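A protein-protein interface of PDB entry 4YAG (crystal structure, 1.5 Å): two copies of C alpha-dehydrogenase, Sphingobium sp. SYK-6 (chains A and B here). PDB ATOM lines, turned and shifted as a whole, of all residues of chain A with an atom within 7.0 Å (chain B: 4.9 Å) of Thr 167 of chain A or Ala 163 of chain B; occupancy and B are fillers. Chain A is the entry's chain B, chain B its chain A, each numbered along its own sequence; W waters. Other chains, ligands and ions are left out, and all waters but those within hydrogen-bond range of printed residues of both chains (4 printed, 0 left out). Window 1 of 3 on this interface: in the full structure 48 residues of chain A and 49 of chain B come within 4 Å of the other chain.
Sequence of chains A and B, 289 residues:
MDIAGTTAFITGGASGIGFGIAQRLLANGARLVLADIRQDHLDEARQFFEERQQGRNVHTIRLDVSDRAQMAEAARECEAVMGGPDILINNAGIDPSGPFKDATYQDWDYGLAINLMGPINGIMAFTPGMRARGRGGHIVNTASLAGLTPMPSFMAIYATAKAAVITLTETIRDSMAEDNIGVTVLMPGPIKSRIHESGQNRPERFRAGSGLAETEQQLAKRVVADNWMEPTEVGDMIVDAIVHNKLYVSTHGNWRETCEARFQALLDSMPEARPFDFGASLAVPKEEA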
ATOM      1  N   GLY A 147     -11.903 -20.009 -16.103  1.00  0.00           N
ATOM      2  CA  GLY A 147     -12.378 -19.703 -17.432  1.00  0.00           C
ATOM      3  C   GLY A 147     -11.247 -19.409 -18.397  1.00  0.00           C
ATOM      4  O   GLY A 147     -11.487 -19.211 -19.584  1.00  0.00           O
ATOM      5  N   ALA A 159     -16.037 -24.372 -16.186  1.00  0.00           N
ATOM      6  CA  ALA A 159     -15.065 -23.674 -17.019  1.00  0.00           C
ATOM      7  C   ALA A 159     -15.700 -23.110 -18.285  1.00  0.00           C
ATOM      8  O   ALA A 159     -15.398 -21.985 -18.699  1.00  0.00           O
ATOM      9  CB  ALA A 159     -13.923 -24.597 -17.365  1.00  0.00           C
ATOM     10  N   THR A 160     -16.597 -23.873 -18.903  1.00  0.00           N
ATOM     11  CA  THR A 160     -17.244 -23.445 -20.129  1.00  0.00           C
ATOM     12  C   THR A 160     -18.033 -22.154 -19.914  1.00  0.00           C
ATOM     13  O   THR A 160     -17.905 -21.199 -20.683  1.00  0.00           O
ATOM     14  CB  THR A 160     -18.155 -24.588 -20.664  1.00  0.00           C
ATOM     15  OG1 THR A 160     -17.343 -25.724 -21.011  1.00  0.00           O
ATOM     16  CG2 THR A 160     -18.942 -24.171 -21.881  1.00  0.00           C
ATOM     17  N   LYS A 162     -17.618 -19.988 -17.411  1.00  0.00           N
ATOM     18  CA  LYS A 162     -16.792 -18.883 -16.937  1.00  0.00           C
ATOM     19  C   LYS A 162     -15.973 -18.279 -18.081  1.00  0.00           C
ATOM     20  O   LYS A 162     -15.745 -17.074 -18.124  1.00  0.00           O
ATOM     21  CB  LYS A 162     -15.882 -19.345 -15.795  1.00  0.00           C
ATOM     22  CG  LYS A 162     -16.619 -19.680 -14.487  1.00  0.00           C
ATOM     23  CD  LYS A 162     -17.397 -18.506 -13.967  1.00  0.00           C
ATOM     24  CE  LYS A 162     -17.881 -18.750 -12.539  1.00  0.00           C
ATOM     25  NZ  LYS A 162     -18.477 -17.514 -11.988  1.00  0.00           N
ATOM     26  N   ALA A 163     -15.552 -19.109 -19.041  1.00  0.00           N
ATOM     27  CA  ALA A 163     -14.853 -18.581 -20.222  1.00  0.00           C
ATOM     28  C   ALA A 163     -15.802 -17.661 -20.997  1.00  0.00           C
ATOM     29  O   ALA A 163     -15.403 -16.596 -21.489  1.00  0.00           O
ATOM     30  CB  ALA A 163     -14.376 -19.714 -21.127  1.00  0.00           C
ATOM     31  N   ALA A 164     -17.064 -18.056 -21.098  1.00  0.00           N
ATOM     32  CA  ALA A 164     -18.074 -17.253 -21.786  1.00  0.00           C
ATOM     33  C   ALA A 164     -18.270 -15.901 -21.095  1.00  0.00           C
ATOM     34  O   ALA A 164     -18.472 -14.891 -21.754  1.00  0.00           O
ATOM     35  CB  ALA A 164     -19.391 -18.011 -21.892  1.00  0.00           C
ATOM     36  N   VAL A 165     -18.189 -15.883 -19.763  1.00  0.00           N
ATOM     37  CA  VAL A 165     -18.384 -14.626 -19.029  1.00  0.00           C
ATOM     38  C   VAL A 165     -17.251 -13.646 -19.300  1.00  0.00           C
ATOM     39  O   VAL A 165     -17.476 -12.438 -19.433  1.00  0.00           O
ATOM     40  CB  VAL A 165     -18.559 -14.883 -17.515  1.00  0.00           C
ATOM     41  CG1 VAL A 165     -18.565 -13.558 -16.735  1.00  0.00           C
ATOM     42  CG2 VAL A 165     -19.851 -15.633 -17.235  1.00  0.00           C
ATOM     43  N   ILE A 166     -16.034 -14.156 -19.442  1.00  0.00           N
ATOM     44  CA  ILE A 166     -14.897 -13.304 -19.766  1.00  0.00           C
ATOM     45  C   ILE A 166     -15.161 -12.639 -21.116  1.00  0.00           C
ATOM     46  O   ILE A 166     -15.064 -11.418 -21.264  1.00  0.00           O
ATOM     47  CB  ILE A 166     -13.562 -14.108 -19.773  1.00  0.00           C
ATOM     48  CG1 ILE A 166     -13.262 -14.616 -18.360  1.00  0.00           C
ATOM     49  CG2 ILE A 166     -12.411 -13.267 -20.345  1.00  0.00           C
ATOM     50  CD1 ILE A 166     -12.096 -15.597 -18.256  1.00  0.00           C
ATOM     51  N   THR A 167     -15.509 -13.448 -22.119  1.00  0.00           N
ATOM     52  CA  THR A 167     -15.740 -12.925 -23.457  1.00  0.00           C
ATOM     53  C   THR A 167     -16.953 -11.996 -23.518  1.00  0.00           C
ATOM     54  O   THR A 167     -16.928 -10.968 -24.223  1.00  0.00           O
ATOM     55  CB  THR A 167     -15.879 -14.100 -24.449  1.00  0.00           C
ATOM     56  OG1 THR A 167     -14.659 -14.840 -24.407  1.00  0.00           O
ATOM     57  CG2 THR A 167     -16.144 -13.605 -25.837  1.00  0.00           C
ATOM     58  N   LEU A 168     -18.015 -12.355 -22.816  1.00  0.00           N
ATOM     59  CA  LEU A 168     -19.197 -11.498 -22.727  1.00  0.00           C
ATOM     60  C   LEU A 168     -18.796 -10.107 -22.280  1.00  0.00           C
ATOM     61  O   LEU A 168     -19.204  -9.090 -22.838  1.00  0.00           O
ATOM     62  CB  LEU A 168     -20.181 -12.106 -21.739  1.00  0.00           C
ATOM     63  CG  LEU A 168     -21.342 -11.215 -21.286  1.00  0.00           C
ATOM     64  CD1 LEU A 168     -22.327 -11.011 -22.415  1.00  0.00           C
ATOM     65  CD2 LEU A 168     -22.013 -11.854 -20.100  1.00  0.00           C
ATOM     66  N   THR A 169     -17.973 -10.079 -21.243  1.00  0.00           N
ATOM     67  CA  THR A 169     -17.571  -8.795 -20.669  1.00  0.00           C
ATOM     68  C   THR A 169     -16.725  -7.977 -21.646  1.00  0.00           C
ATOM     69  O   THR A 169     -16.932  -6.769 -21.819  1.00  0.00           O
ATOM     70  CB  THR A 169     -16.805  -8.988 -19.357  1.00  0.00           C
ATOM     71  OG1 THR A 169     -17.563  -9.829 -18.493  1.00  0.00           O
ATOM     72  CG2 THR A 169     -16.571  -7.645 -18.664  1.00  0.00           C
ATOM     73  N   GLU A 170     -15.752  -8.620 -22.278  1.00  0.00           N
ATOM     74  CA  GLU A 170     -14.954  -7.934 -23.293  1.00  0.00           C
ATOM     75  C   GLU A 170     -15.829  -7.347 -24.394  1.00  0.00           C
ATOM     76  O   GLU A 170     -15.615  -6.215 -24.829  1.00  0.00           O
ATOM     77  CB  GLU A 170     -13.955  -8.905 -23.932  1.00  0.00           C
ATOM     78  CG  GLU A 170     -12.925  -9.464 -23.011  1.00  0.00           C
ATOM     79  CD  GLU A 170     -12.143 -10.632 -23.616  1.00  0.00           C
ATOM     80  OE1 GLU A 170     -12.590 -11.194 -24.644  1.00  0.00           O
ATOM     81  OE2 GLU A 170     -11.097 -10.998 -23.041  1.00  0.00           O
ATOM     82  N   THR A 171     -16.774  -8.128 -24.902  1.00  0.00           N
ATOM     83  CA  THR A 171     -17.540  -7.702 -26.063  1.00  0.00           C
ATOM     84  C   THR A 171     -18.512  -6.582 -25.776  1.00  0.00           C
ATOM     85  O   THR A 171     -18.717  -5.720 -26.628  1.00  0.00           O
ATOM     86  CB  THR A 171     -18.298  -8.887 -26.733  1.00  0.00           C
ATOM     87  OG1 THR A 171     -19.338  -9.397 -25.869  1.00  0.00           O
ATOM     88  CG2 THR A 171     -17.324  -9.967 -27.083  1.00  0.00           C
ATOM     89  N   ILE A 172     -19.112  -6.565 -24.587  1.00  0.00           N
ATOM     90  CA  ILE A 172     -20.086  -5.520 -24.291  1.00  0.00           C
ATOM     91  C   ILE A 172     -19.435  -4.171 -23.985  1.00  0.00           C
ATOM     92  O   ILE A 172     -20.127  -3.148 -23.970  1.00  0.00           O
ATOM     93  CB  ILE A 172     -21.043  -5.873 -23.128  1.00  0.00           C
ATOM     94  CG1 ILE A 172     -20.296  -5.945 -21.795  1.00  0.00           C
ATOM     95  CG2 ILE A 172     -21.833  -7.159 -23.447  1.00  0.00           C
ATOM     96  CD1 ILE A 172     -21.221  -6.218 -20.579  1.00  0.00           C
ATOM     97  N   ARG A 173     -18.126  -4.155 -23.759  1.00  0.00           N
ATOM     98  CA  ARG A 173     -17.461  -2.925 -23.283  1.00  0.00           C
ATOM     99  C   ARG A 173     -17.797  -1.718 -24.157  1.00  0.00           C
ATOM    100  O   ARG A 173     -18.160  -0.641 -23.646  1.00  0.00           O
ATOM    101  CB  ARG A 173     -15.941  -3.098 -23.208  1.00  0.00           C
ATOM    102  CG  ARG A 173     -15.223  -1.950 -22.504  1.00  0.00           C
ATOM    103  CD  ARG A 173     -13.744  -2.153 -22.510  1.00  0.00           C
ATOM    104  NE  ARG A 173     -13.121  -1.496 -21.373  1.00  0.00           N
ATOM    105  CZ  ARG A 173     -11.815  -1.373 -21.206  1.00  0.00           C
ATOM    106  NH1 ARG A 173     -10.960  -1.844 -22.108  1.00  0.00           N
ATOM    107  NH2 ARG A 173     -11.373  -0.780 -20.123  1.00  0.00           N
ATOM    108  N   VAL A 185     -14.328  -7.681 -15.770  1.00  0.00           N
ATOM    109  CA  VAL A 185     -14.480  -9.084 -15.424  1.00  0.00           C
ATOM    110  C   VAL A 185     -13.458  -9.453 -14.341  1.00  0.00           C
ATOM    111  O   VAL A 185     -12.258  -9.235 -14.489  1.00  0.00           O
ATOM    112  CB  VAL A 185     -14.428 -10.026 -16.638  1.00  0.00           C
ATOM    113  CG1 VAL A 185     -13.109  -9.938 -17.384  1.00  0.00           C
ATOM    114  CG2 VAL A 185     -14.678 -11.443 -16.162  1.00  0.00           C
ATOM    115  N   ARG A 262      -1.132 -22.326 -22.543  1.00  0.00           N
ATOM    116  CA  ARG A 262      -2.336 -22.444 -23.330  1.00  0.00           C
ATOM    117  C   ARG A 262      -2.298 -21.442 -24.476  1.00  0.00           C
ATOM    118  O   ARG A 262      -2.576 -21.783 -25.614  1.00  0.00           O
ATOM    119  CB  ARG A 262      -3.577 -22.182 -22.465  1.00  0.00           C
ATOM    120  CG  ARG A 262      -4.883 -22.272 -23.201  1.00  0.00           C
ATOM    121  CD  ARG A 262      -6.092 -21.762 -22.416  1.00  0.00           C
ATOM    122  NE  ARG A 262      -7.254 -21.783 -23.300  1.00  0.00           N
ATOM    123  CZ  ARG A 262      -8.200 -20.857 -23.348  1.00  0.00           C
ATOM    124  NH1 ARG A 262      -8.192 -19.820 -22.529  1.00  0.00           N
ATOM    125  NH2 ARG A 262      -9.177 -20.985 -24.230  1.00  0.00           N
ATOM    126  N   GLY B 147     -13.926 -16.347 -31.085  1.00  0.00           N
ATOM    127  CA  GLY B 147     -14.013 -16.786 -29.712  1.00  0.00           C
ATOM    128  C   GLY B 147     -12.728 -16.536 -28.961  1.00  0.00           C
ATOM    129  O   GLY B 147     -12.674 -16.787 -27.757  1.00  0.00           O
ATOM    130  N   ALA B 159     -19.503 -14.205 -30.236  1.00  0.00           N
ATOM    131  CA  ALA B 159     -18.218 -14.382 -29.575  1.00  0.00           C
ATOM    132  C   ALA B 159     -18.324 -15.156 -28.271  1.00  0.00           C
ATOM    133  O   ALA B 159     -17.479 -15.995 -27.965  1.00  0.00           O
ATOM    134  CB  ALA B 159     -17.591 -13.054 -29.314  1.00  0.00           C
ATOM    135  N   THR B 160     -19.343 -14.826 -27.487  1.00  0.00           N
ATOM    136  CA  THR B 160     -19.557 -15.442 -26.187  1.00  0.00           C
ATOM    137  C   THR B 160     -19.725 -16.954 -26.326  1.00  0.00           C
ATOM    138  O   THR B 160     -19.119 -17.738 -25.617  1.00  0.00           O
ATOM    139  CB  THR B 160     -20.781 -14.798 -25.484  1.00  0.00           C
ATOM    140  OG1 THR B 160     -20.515 -13.411 -25.213  1.00  0.00           O
ATOM    141  CG2 THR B 160     -21.124 -15.483 -24.176  1.00  0.00           C
ATOM    142  N   ALA B 161     -20.567 -17.365 -27.278  1.00  0.00           N
ATOM    143  CA  ALA B 161     -20.783 -18.792 -27.517  1.00  0.00           C
ATOM    144  C   ALA B 161     -19.537 -19.471 -28.035  1.00  0.00           C
ATOM    145  O   ALA B 161     -19.206 -20.578 -27.615  1.00  0.00           O
ATOM    146  CB  ALA B 161     -21.920 -18.985 -28.528  1.00  0.00           C
ATOM    147  N   LYS B 162     -18.849 -18.825 -28.958  1.00  0.00           N
ATOM    148  CA  LYS B 162     -17.685 -19.443 -29.568  1.00  0.00           C
ATOM    149  C   LYS B 162     -16.519 -19.603 -28.593  1.00  0.00           C
ATOM    150  O   LYS B 162     -15.782 -20.576 -28.666  1.00  0.00           O
ATOM    151  CB  LYS B 162     -17.256 -18.692 -30.827  1.00  0.00           C
ATOM    152  CG  LYS B 162     -18.294 -18.757 -31.976  1.00  0.00           C
ATOM    153  CD  LYS B 162     -18.463 -20.170 -32.456  1.00  0.00           C
ATOM    154  CE  LYS B 162     -19.226 -20.259 -33.781  1.00  0.00           C
ATOM    155  NZ  LYS B 162     -19.384 -21.658 -34.212  1.00  0.00           N
ATOM    156  N   ALA B 163     -16.329 -18.640 -27.689  1.00  0.00           N
ATOM    157  CA  ALA B 163     -15.328 -18.795 -26.634  1.00  0.00           C
ATOM    158  C   ALA B 163     -15.631 -20.010 -25.770  1.00  0.00           C
ATOM    159  O   ALA B 163     -14.745 -20.784 -25.396  1.00  0.00           O
ATOM    160  CB  ALA B 163     -15.277 -17.555 -25.770  1.00  0.00           C
ATOM    161  N   ALA B 164     -16.908 -20.178 -25.449  1.00  0.00           N
ATOM    162  CA  ALA B 164     -17.340 -21.310 -24.648  1.00  0.00           C
ATOM    163  C   ALA B 164     -17.043 -22.641 -25.344  1.00  0.00           C
ATOM    164  O   ALA B 164     -16.679 -23.605 -24.693  1.00  0.00           O
ATOM    165  CB  ALA B 164     -18.812 -21.214 -24.315  1.00  0.00           C
ATOM    166  N   VAL B 165     -17.230 -22.697 -26.658  1.00  0.00           N
ATOM    167  CA  VAL B 165     -16.951 -23.930 -27.381  1.00  0.00           C
ATOM    168  C   VAL B 165     -15.474 -24.306 -27.325  1.00  0.00           C
ATOM    169  O   VAL B 165     -15.111 -25.487 -27.245  1.00  0.00           O
ATOM    170  CB  VAL B 165     -17.429 -23.805 -28.850  1.00  0.00           C
ATOM    171  CG1 VAL B 165     -16.978 -25.021 -29.681  1.00  0.00           C
ATOM    172  CG2 VAL B 165     -18.930 -23.681 -28.882  1.00  0.00           C
ATOM    173  N   ILE B 166     -14.600 -23.311 -27.379  1.00  0.00           N
ATOM    174  CA  ILE B 166     -13.185 -23.587 -27.273  1.00  0.00           C
ATOM    175  C   ILE B 166     -12.888 -24.243 -25.908  1.00  0.00           C
ATOM    176  O   ILE B 166     -12.241 -25.278 -25.823  1.00  0.00           O
ATOM    177  CB  ILE B 166     -12.355 -22.301 -27.462  1.00  0.00           C
ATOM    178  CG1 ILE B 166     -12.537 -21.751 -28.887  1.00  0.00           C
ATOM    179  CG2 ILE B 166     -10.900 -22.581 -27.142  1.00  0.00           C
ATOM    180  CD1 ILE B 166     -11.970 -20.344 -29.077  1.00  0.00           C
ATOM    181  N   THR B 167     -13.373 -23.621 -24.831  1.00  0.00           N
ATOM    182  CA  THR B 167     -13.128 -24.134 -23.482  1.00  0.00           C
ATOM    183  C   THR B 167     -13.784 -25.502 -23.288  1.00  0.00           C
ATOM    184  O   THR B 167     -13.201 -26.394 -22.689  1.00  0.00           O
ATOM    185  CB  THR B 167     -13.627 -23.127 -22.453  1.00  0.00           C
ATOM    186  OG1 THR B 167     -12.893 -21.908 -22.636  1.00  0.00           O
ATOM    187  CG2 THR B 167     -13.436 -23.631 -21.020  1.00  0.00           C
ATOM    188  N   ARG B 262      -4.420  -9.302 -26.428  1.00  0.00           N
ATOM    189  CA  ARG B 262      -5.420  -9.750 -25.451  1.00  0.00           C
ATOM    190  C   ARG B 262      -4.765 -10.605 -24.360  1.00  0.00           C
ATOM    191  O   ARG B 262      -4.970 -10.388 -23.159  1.00  0.00           O
ATOM    192  CB  ARG B 262      -6.522 -10.562 -26.140  1.00  0.00           C
ATOM    193  CG  ARG B 262      -7.621 -11.005 -25.201  1.00  0.00           C
ATOM    194  CD  ARG B 262      -8.548 -12.043 -25.787  1.00  0.00           C
ATOM    195  NE  ARG B 262      -9.447 -12.474 -24.735  1.00  0.00           N
ATOM    196  CZ  ARG B 262      -9.895 -13.702 -24.549  1.00  0.00           C
ATOM    197  NH1 ARG B 262      -9.613 -14.675 -25.404  1.00  0.00           N
ATOM    198  NH2 ARG B 262     -10.660 -13.945 -23.494  1.00  0.00           N
HETATM  199  O   HOH W   1     -12.731 -13.710 -25.903  1.00  0.00           O
HETATM  200  O   HOH W   2     -11.880 -19.810 -24.418  1.00  0.00           O
HETATM  201  O   HOH W   3     -10.391 -22.023 -21.573  1.00  0.00           O
HETATM  202  O   HOH W   4     -12.547 -16.215 -22.967  1.00  0.00           O
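The side-chain carboxylate (OE2) of Glu 170 of chain A is in salt-bridge range of the guanidinium group (NE) of Arg 262 of chain B, 2.8 Å away.
OG1 of Thr 167 of chain A lies within hydrogen-bond range of O of Ala 163 of chain A (3.5 Å). The side-chain hydroxyl (OG1) of Thr 171 of chain A sits close to the backbone carbonyl oxygen (O) of Thr 167 of chain A (3.3 Å). O of Leu 168 of chain A lies within hydrogen-bond range of OG1 of Thr 171 of chain A (3.0 Å).
Of the printed residues of chain B, Ala 163 of chain A touches Thr 167. Printed residues of chain B within 4 Å of Thr 167 of chain A: Ala 159, Thr 160 and Ala 163. Thr 169 of chain A touches none of the printed residues of chain B. Printed residues of chain B within 4 Å of Thr 171 of chain A: Ala 159 (3.8 Å). Printed residues of chain B within 4 Å of Arg 262 of chain A: Ile 166. Printed residues of chain A within 4 Å of Ala 159 of chain B: Thr 167 (3.5 Å) and Thr 171 (3.8 Å). Of the printed residues of chain A, Ala 163 of chain B touches Thr 167 (3.1 Å). The nearest residue of chain A that does not touch Ala 163 of chain B is Ala 163 of chain A (4.4 Å).
Among the printed residues, merely in contact across the chains: Ala 159 of chain A with Thr 167 of chain B, Thr 160 of chain A with Ala 164 of chain B, Thr 160 of chain A with Thr 167 of chain B, Ala 163 of chain A with Thr 167 of chain B, Ala 164 of chain A with Thr 160 of chain B, Ile 166 of chain A with Arg 262 of chain B, Thr 167 of chain A with Ala 159 of chain B, Thr 167 of chain A with Thr 160 of chain B, Thr 167 of chain A with Ala 163 of chain B, Leu 168 of chain A with Thr 160 of chain B, Thr 171 of chain A with Ala 159 of chain B and Arg 262 of chain A with Ile 166 of chain B.
Of the 17 printed residues of chain A, 10 touch a printed residue of chain B. Printed residues of chain A that touch a printed residue of chain B: Ala 159, Thr 160, Ala 163, Ala 164, Ile 166, Thr 167, Leu 168, Glu 170, Thr 171 and Arg 262. Hydrophobic or aromatic side chains of chain A that line the printed part of chain B: Ala 159, Ala 163, Ala 164, Ile 166 and Leu 168. Of the 11 printed residues of chain B, 7 touch a printed residue of chain A. Among the printed residues, 13 pairs touch across the chains.
Ala 159 of chain A touches Thr 167 of chain B, and with the chains exchanged Thr 167 of chain A touches Ala 159 of chain B. Thr 160 of chain A touches Ala 164 of chain B, and with the chains exchanged Ala 164 of chain A touches Thr 160 of chain B. Ala 163 of chain A touches Thr 167 of chain B, and with the chains exchanged Thr 167 of chain A touches Ala 163 of chain B. Ile 166 of chain A touches Arg 262 of chain B, and with the chains exchanged Arg 262 of chain A touches Ile 166 of chain B. Of the 13 pairs that touch across the chains among the printed residues, 10 have their exchanged pair printed and touching as well.
Water W1 lies within hydrogen-bond range of OG1 of Thr 167 of chain A, OE1 of Glu 170 of chain A and NH2 of Arg 262 of chain B. Water W3 lies within hydrogen-bond range of the side-chain hydroxyl (OG1) of Thr 167 of chain B and the guanidinium group (NH2) of Arg 262 of chain A. Water W4 lies within hydrogen-bond range of the side-chain hydroxyl of Thr 167 of chain A, the guanidinium group of Arg 262 of chain B and the backbone carbonyl oxygen of Ala 163 of chain A. Water W2 lies within hydrogen-bond range of the side-chain hydroxyl of Thr 167 of chain B (2.9 Å), the guanidinium group of Arg 262 of chain A (3.0 Å) and the backbone carbonyl oxygen of Ala 163 of chain B (3.2 Å).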
